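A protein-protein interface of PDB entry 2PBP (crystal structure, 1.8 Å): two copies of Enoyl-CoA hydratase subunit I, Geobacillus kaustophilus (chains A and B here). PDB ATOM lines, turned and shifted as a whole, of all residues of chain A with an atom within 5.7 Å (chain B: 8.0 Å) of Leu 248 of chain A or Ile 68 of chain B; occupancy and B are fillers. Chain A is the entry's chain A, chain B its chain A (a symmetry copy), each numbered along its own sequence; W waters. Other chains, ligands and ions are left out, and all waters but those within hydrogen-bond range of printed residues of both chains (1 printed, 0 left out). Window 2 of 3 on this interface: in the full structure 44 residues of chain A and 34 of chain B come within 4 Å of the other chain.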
ATOM      1  N   GLY A 243      -5.876   8.453 -13.559  1.00  0.00           N
ATOM      2  CA  GLY A 243      -4.646   7.870 -14.066  1.00  0.00           C
ATOM      3  C   GLY A 243      -4.218   8.434 -15.409  1.00  0.00           C
ATOM      4  O   GLY A 243      -3.044   8.734 -15.625  1.00  0.00           O
ATOM      5  N   MET A 244      -5.173   8.591 -16.317  1.00  0.00           N
ATOM      6  CA  MET A 244      -4.857   9.107 -17.639  1.00  0.00           C
ATOM      7  C   MET A 244      -4.589  10.610 -17.640  1.00  0.00           C
ATOM      8  O   MET A 244      -3.767  11.093 -18.418  1.00  0.00           O
ATOM      9  CB  MET A 244      -5.974   8.733 -18.615  1.00  0.00           C
ATOM     10  CG  MET A 244      -6.119   7.217 -18.730  1.00  0.00           C
ATOM     11  SD  MET A 244      -7.280   6.629 -19.962  1.00  0.00           S
ATOM     12  CE  MET A 244      -7.048   4.850 -19.807  1.00  0.00           C
ATOM     13  N   ALA A 245      -5.262  11.350 -16.763  1.00  0.00           N
ATOM     14  CA  ALA A 245      -5.030  12.789 -16.687  1.00  0.00           C
ATOM     15  C   ALA A 245      -3.638  13.017 -16.089  1.00  0.00           C
ATOM     16  O   ALA A 245      -2.894  13.891 -16.533  1.00  0.00           O
ATOM     17  CB  ALA A 245      -6.095  13.461 -15.822  1.00  0.00           C
ATOM     18  N   ALA A 246      -3.293  12.218 -15.083  1.00  0.00           N
ATOM     19  CA  ALA A 246      -1.993  12.326 -14.426  1.00  0.00           C
ATOM     20  C   ALA A 246      -0.866  12.001 -15.401  1.00  0.00           C
ATOM     21  O   ALA A 246       0.185  12.642 -15.383  1.00  0.00           O
ATOM     22  CB  ALA A 246      -1.928  11.384 -13.225  1.00  0.00           C
ATOM     23  N   PHE A 247      -1.085  10.999 -16.245  1.00  0.00           N
ATOM     24  CA  PHE A 247      -0.076  10.608 -17.223  1.00  0.00           C
ATOM     25  C   PHE A 247       0.188  11.741 -18.211  1.00  0.00           C
ATOM     26  O   PHE A 247       1.339  12.045 -18.527  1.00  0.00           O
ATOM     27  CB  PHE A 247      -0.526   9.370 -17.994  1.00  0.00           C
ATOM     28  CG  PHE A 247       0.546   8.792 -18.872  1.00  0.00           C
ATOM     29  CD1 PHE A 247       1.603   8.078 -18.318  1.00  0.00           C
ATOM     30  CD2 PHE A 247       0.510   8.979 -20.251  1.00  0.00           C
ATOM     31  CE1 PHE A 247       2.614   7.558 -19.126  1.00  0.00           C
ATOM     32  CE2 PHE A 247       1.517   8.463 -21.066  1.00  0.00           C
ATOM     33  CZ  PHE A 247       2.569   7.751 -20.501  1.00  0.00           C
ATOM     34  N   LEU A 248      -0.887  12.354 -18.702  1.00  0.00           N
ATOM     35  CA  LEU A 248      -0.782  13.454 -19.659  1.00  0.00           C
ATOM     36  C   LEU A 248      -0.136  14.686 -19.034  1.00  0.00           C
ATOM     37  O   LEU A 248       0.608  15.410 -19.694  1.00  0.00           O
ATOM     38  CB  LEU A 248      -2.168  13.834 -20.189  1.00  0.00           C
ATOM     39  CG  LEU A 248      -2.882  12.835 -21.100  1.00  0.00           C
ATOM     40  CD1 LEU A 248      -4.236  13.401 -21.502  1.00  0.00           C
ATOM     41  CD2 LEU A 248      -2.032  12.561 -22.335  1.00  0.00           C
ATOM     42  N   GLU A 249      -0.428  14.920 -17.759  1.00  0.00           N
ATOM     43  CA  GLU A 249       0.119  16.070 -17.055  1.00  0.00           C
ATOM     44  C   GLU A 249       1.508  15.792 -16.498  1.00  0.00           C
ATOM     45  O   GLU A 249       2.138  16.672 -15.915  1.00  0.00           O
ATOM     46  CB  GLU A 249      -0.822  16.479 -15.924  1.00  0.00           C
ATOM     47  CG  GLU A 249      -2.099  17.144 -16.410  1.00  0.00           C
ATOM     48  CD  GLU A 249      -3.094  17.366 -15.294  1.00  0.00           C
ATOM     49  OE1 GLU A 249      -2.665  17.719 -14.177  1.00  0.00           O
ATOM     50  OE2 GLU A 249      -4.307  17.201 -15.537  1.00  0.00           O
ATOM     51  N   LYS A 250       1.978  14.564 -16.686  1.00  0.00           N
ATOM     52  CA  LYS A 250       3.288  14.150 -16.208  1.00  0.00           C
ATOM     53  C   LYS A 250       3.447  14.364 -14.705  1.00  0.00           C
ATOM     54  O   LYS A 250       4.446  14.927 -14.244  1.00  0.00           O
ATOM     55  CB  LYS A 250       4.393  14.895 -16.966  1.00  0.00           C
ATOM     56  CG  LYS A 250       4.331  14.706 -18.477  1.00  0.00           C
ATOM     57  CD  LYS A 250       5.654  15.041 -19.155  1.00  0.00           C
ATOM     58  CE  LYS A 250       6.145  16.433 -18.788  1.00  0.00           C
ATOM     59  NZ  LYS A 250       5.138  17.480 -19.110  1.00  0.00           N
ATOM     60  N   ALA B  28       2.008   2.301 -32.012  1.00  0.00           N
ATOM     61  CA  ALA B  28       0.917   2.180 -31.050  1.00  0.00           C
ATOM     62  C   ALA B  28      -0.205   1.300 -31.588  1.00  0.00           C
ATOM     63  O   ALA B  28      -0.708   1.519 -32.692  1.00  0.00           O
ATOM     64  CB  ALA B  28       0.378   3.562 -30.703  1.00  0.00           C
ATOM     65  N   GLY B  65       1.185   0.362 -26.548  1.00  0.00           N
ATOM     66  CA  GLY B  65      -0.253   0.175 -26.478  1.00  0.00           C
ATOM     67  C   GLY B  65      -1.002   1.343 -27.084  1.00  0.00           C
ATOM     68  O   GLY B  65      -0.390   2.321 -27.520  1.00  0.00           O
ATOM     69  N   ALA B  66      -2.326   1.239 -27.126  1.00  0.00           N
ATOM     70  CA  ALA B  66      -3.154   2.307 -27.669  1.00  0.00           C
ATOM     71  C   ALA B  66      -2.859   3.581 -26.889  1.00  0.00           C
ATOM     72  O   ALA B  66      -2.638   3.533 -25.678  1.00  0.00           O
ATOM     73  CB  ALA B  66      -4.631   1.942 -27.546  1.00  0.00           C
ATOM     74  N   ASP B  67      -2.851   4.715 -27.583  1.00  0.00           N
ATOM     75  CA  ASP B  67      -2.566   5.999 -26.949  1.00  0.00           C
ATOM     76  C   ASP B  67      -3.667   6.415 -25.980  1.00  0.00           C
ATOM     77  O   ASP B  67      -4.814   5.978 -26.100  1.00  0.00           O
ATOM     78  CB  ASP B  67      -2.389   7.085 -28.008  1.00  0.00           C
ATOM     79  CG  ASP B  67      -3.592   7.204 -28.915  1.00  0.00           C
ATOM     80  OD1 ASP B  67      -3.750   6.355 -29.820  1.00  0.00           O
ATOM     81  OD2 ASP B  67      -4.390   8.139 -28.711  1.00  0.00           O
ATOM     82  N   ILE B  68      -3.312   7.274 -25.029  1.00  0.00           N
ATOM     83  CA  ILE B  68      -4.264   7.746 -24.031  1.00  0.00           C
ATOM     84  C   ILE B  68      -5.432   8.513 -24.638  1.00  0.00           C
ATOM     85  O   ILE B  68      -6.564   8.393 -24.169  1.00  0.00           O
ATOM     86  CB  ILE B  68      -3.574   8.641 -22.964  1.00  0.00           C
ATOM     87  CG1 ILE B  68      -2.829   7.764 -21.954  1.00  0.00           C
ATOM     88  CG2 ILE B  68      -4.610   9.502 -22.244  1.00  0.00           C
ATOM     89  CD1 ILE B  68      -3.685   6.785 -21.110  1.00  0.00           C
ATOM     90  N   GLN B  69      -5.169   9.301 -25.677  1.00  0.00           N
ATOM     91  CA  GLN B  69      -6.243  10.062 -26.291  1.00  0.00           C
ATOM     92  C   GLN B  69      -7.362   9.142 -26.773  1.00  0.00           C
ATOM     93  O   GLN B  69      -8.539   9.460 -26.616  1.00  0.00           O
ATOM     94  CB  GLN B  69      -5.721  10.906 -27.457  1.00  0.00           C
ATOM     95  CG  GLN B  69      -6.789  11.836 -28.024  1.00  0.00           C
ATOM     96  CD  GLN B  69      -6.225  12.893 -28.948  1.00  0.00           C
ATOM     97  OE1 GLN B  69      -5.345  13.663 -28.564  1.00  0.00           O
ATOM     98  NE2 GLN B  69      -6.735  12.942 -30.172  1.00  0.00           N
ATOM     99  N   GLU B  70      -7.001   7.999 -27.349  1.00  0.00           N
ATOM    100  CA  GLU B  70      -8.013   7.062 -27.829  1.00  0.00           C
ATOM    101  C   GLU B  70      -8.719   6.378 -26.659  1.00  0.00           C
ATOM    102  O   GLU B  70      -9.944   6.233 -26.660  1.00  0.00           O
ATOM    103  CB  GLU B  70      -7.381   6.015 -28.751  1.00  0.00           C
ATOM    104  CG  GLU B  70      -8.343   4.914 -29.189  1.00  0.00           C
ATOM    105  CD  GLU B  70      -7.843   4.143 -30.399  1.00  0.00           C
ATOM    106  OE1 GLU B  70      -7.739   4.748 -31.485  1.00  0.00           O
ATOM    107  OE2 GLU B  70      -7.555   2.936 -30.263  1.00  0.00           O
ATOM    108  N   MET B  71      -7.949   5.971 -25.657  1.00  0.00           N
ATOM    109  CA  MET B  71      -8.522   5.304 -24.492  1.00  0.00           C
ATOM    110  C   MET B  71      -9.394   6.228 -23.650  1.00  0.00           C
ATOM    111  O   MET B  71     -10.391   5.792 -23.078  1.00  0.00           O
ATOM    112  CB  MET B  71      -7.420   4.721 -23.602  1.00  0.00           C
ATOM    113  CG  MET B  71      -6.595   3.622 -24.246  1.00  0.00           C
ATOM    114  SD  MET B  71      -5.624   2.716 -23.016  1.00  0.00           S
ATOM    115  CE  MET B  71      -4.244   3.820 -22.765  1.00  0.00           C
ATOM    116  N   ALA B  72      -9.018   7.501 -23.572  1.00  0.00           N
ATOM    117  CA  ALA B  72      -9.765   8.467 -22.773  1.00  0.00           C
ATOM    118  C   ALA B  72     -11.177   8.702 -23.296  1.00  0.00           C
ATOM    119  O   ALA B  72     -12.035   9.190 -22.568  1.00  0.00           O
ATOM    120  CB  ALA B  72      -9.004   9.791 -22.706  1.00  0.00           C
ATOM    121  N   LYS B  73     -11.416   8.357 -24.557  1.00  0.00           N
ATOM    122  CA  LYS B  73     -12.737   8.534 -25.152  1.00  0.00           C
ATOM    123  C   LYS B  73     -13.714   7.447 -24.716  1.00  0.00           C
ATOM    124  O   LYS B  73     -14.929   7.603 -24.838  1.00  0.00           O
ATOM    125  CB  LYS B  73     -12.644   8.497 -26.677  1.00  0.00           C
ATOM    126  CG  LYS B  73     -11.857   9.623 -27.316  1.00  0.00           C
ATOM    127  CD  LYS B  73     -11.846   9.454 -28.832  1.00  0.00           C
ATOM    128  CE  LYS B  73     -13.265   9.404 -29.394  1.00  0.00           C
ATOM    129  NZ  LYS B  73     -13.289   9.111 -30.856  1.00  0.00           N
ATOM    130  N   ASP B  74     -13.179   6.343 -24.208  1.00  0.00           N
ATOM    131  CA  ASP B  74     -14.014   5.217 -23.814  1.00  0.00           C
ATOM    132  C   ASP B  74     -14.703   5.253 -22.453  1.00  0.00           C
ATOM    133  O   ASP B  74     -14.311   5.985 -21.545  1.00  0.00           O
ATOM    134  CB  ASP B  74     -13.202   3.923 -23.923  1.00  0.00           C
ATOM    135  CG  ASP B  74     -12.641   3.702 -25.317  1.00  0.00           C
ATOM    136  OD1 ASP B  74     -13.342   4.031 -26.298  1.00  0.00           O
ATOM    137  OD2 ASP B  74     -11.507   3.185 -25.433  1.00  0.00           O
ATOM    138  N   GLU B 132      -0.353  -0.631 -18.118  1.00  0.00           N
ATOM    139  CA  GLU B 132      -1.769  -0.273 -18.020  1.00  0.00           C
ATOM    140  C   GLU B 132      -2.224   0.044 -16.603  1.00  0.00           C
ATOM    141  O   GLU B 132      -3.009   0.969 -16.391  1.00  0.00           O
ATOM    142  CB  GLU B 132      -2.666  -1.386 -18.583  1.00  0.00           C
ATOM    143  CG  GLU B 132      -2.635  -1.521 -20.093  1.00  0.00           C
ATOM    144  CD  GLU B 132      -1.694  -2.612 -20.561  1.00  0.00           C
ATOM    145  OE1 GLU B 132      -0.628  -2.786 -19.938  1.00  0.00           O
ATOM    146  OE2 GLU B 132      -2.016  -3.289 -21.562  1.00  0.00           O
ATOM    147  N   ASN B 134      -0.752   1.497 -14.236  1.00  0.00           N
ATOM    148  CA  ASN B 134      -0.394   2.837 -13.791  1.00  0.00           C
ATOM    149  C   ASN B 134      -1.328   3.913 -14.328  1.00  0.00           C
ATOM    150  O   ASN B 134      -1.283   5.064 -13.885  1.00  0.00           O
ATOM    151  CB  ASN B 134       1.058   3.154 -14.160  1.00  0.00           C
ATOM    152  CG  ASN B 134       2.040   2.240 -13.456  1.00  0.00           C
ATOM    153  OD1 ASN B 134       1.869   1.924 -12.278  1.00  0.00           O
ATOM    154  ND2 ASN B 134       3.076   1.817 -14.167  1.00  0.00           N
ATOM    155  N   LEU B 135      -2.185   3.536 -15.271  1.00  0.00           N
ATOM    156  CA  LEU B 135      -3.141   4.473 -15.842  1.00  0.00           C
ATOM    157  C   LEU B 135      -4.505   4.252 -15.200  1.00  0.00           C
ATOM    158  O   LEU B 135      -5.482   4.905 -15.560  1.00  0.00           O
ATOM    159  CB  LEU B 135      -3.256   4.269 -17.357  1.00  0.00           C
ATOM    160  CG  LEU B 135      -1.998   4.483 -18.198  1.00  0.00           C
ATOM    161  CD1 LEU B 135      -2.330   4.243 -19.664  1.00  0.00           C
ATOM    162  CD2 LEU B 135      -1.465   5.894 -17.995  1.00  0.00           C
ATOM    163  N   GLY B 136      -4.565   3.324 -14.249  1.00  0.00           N
ATOM    164  CA  GLY B 136      -5.826   3.036 -13.589  1.00  0.00           C
ATOM    165  C   GLY B 136      -6.622   1.928 -14.265  1.00  0.00           C
ATOM    166  O   GLY B 136      -7.743   1.625 -13.851  1.00  0.00           O
ATOM    167  N   VAL B 137      -6.058   1.319 -15.304  1.00  0.00           N
ATOM    168  CA  VAL B 137      -6.753   0.242 -16.004  1.00  0.00           C
ATOM    169  C   VAL B 137      -5.981  -1.083 -15.947  1.00  0.00           C
ATOM    170  O   VAL B 137      -5.257  -1.332 -14.982  1.00  0.00           O
ATOM    171  CB  VAL B 137      -7.061   0.637 -17.476  1.00  0.00           C
ATOM    172  CG1 VAL B 137      -8.068   1.784 -17.501  1.00  0.00           C
ATOM    173  CG2 VAL B 137      -5.788   1.049 -18.196  1.00  0.00           C
HETATM  174  O   HOH W   1      -0.976   7.810 -14.203  1.00  0.00           O
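The backbone carbonyl oxygen of Glu 132 of chain B is in hydrogen-bond range of the backbone NH of Val 137 of chain B (3.3 Å).
Gly 243 of chain A touches Leu 135 of chain B.
Met 244 of chain A touches Ile 68 of chain B (CG to CD1, 3.4 Å).
CE of Met 244 of chain A touches CB of Met 71 of chain B, 3.8 Å away.
O of Leu 135 of chain B touches N of Met 244 of chain A, 3.8 Å away.
CE of Met 244 of chain A touches CG1 of Val 137 of chain B, at 3.97 Å.
Ile 68 of chain B touches Phe 247 of chain A.
Phe 247 of chain A touches Leu 135 of chain B.
Ile 68 of chain B touches Leu 248 of chain A.
Leu 248 of chain A touches one residue of chain B.
Printed residues of chain A within 4 Å of Ile 68 of chain B: Met 244, Phe 247 and Leu 248.
Printed residues of chain A within 4 Å of Val 137 of chain B: Met 244 (3.97 Å).
Of the printed residues of chain B, Phe 247 of chain A touches Ile 68 and Leu 135.
Gly 65 of chain B touches none of the printed residues of chain A.
The nearest residue of chain B that does not touch Leu 248 of chain A is Gln 69 of chain B (5.6 Å).
The nearest printed residue of chain A that does not touch Ile 68 of chain B is Ala 245 of chain A (5.8 Å).
The nearest printed residue of chain A that does not touch Met 71 of chain B is Phe 247 of chain A (7.5 Å).
Hydrophobic or aromatic side chains of chain A within 4 Å of the printed part of chain B: Met 244, Phe 247 and Leu 248.
Of the 16 printed residues of chain B, 4 touch a printed residue of chain A.
Printed residues of chain B that touch a printed residue of chain A: Ile 68, Met 71, Leu 135 and Val 137.
Hydrophobic or aromatic side chains of chain B that line the printed part of chain A: Ile 68, Met 71, Leu 135 and Val 137.
Among the printed residues, 8 pairs touch across the chains.
No position is printed for both chains.
Of the 8 pairs that touch across the chains among the printed residues, none has its exchanged pair printed and touching as well.
Water W1 lies within hydrogen-bond range of O of Gly 243 of chain A (2.7 Å) and O of Asn 134 of chain B (2.8 Å).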
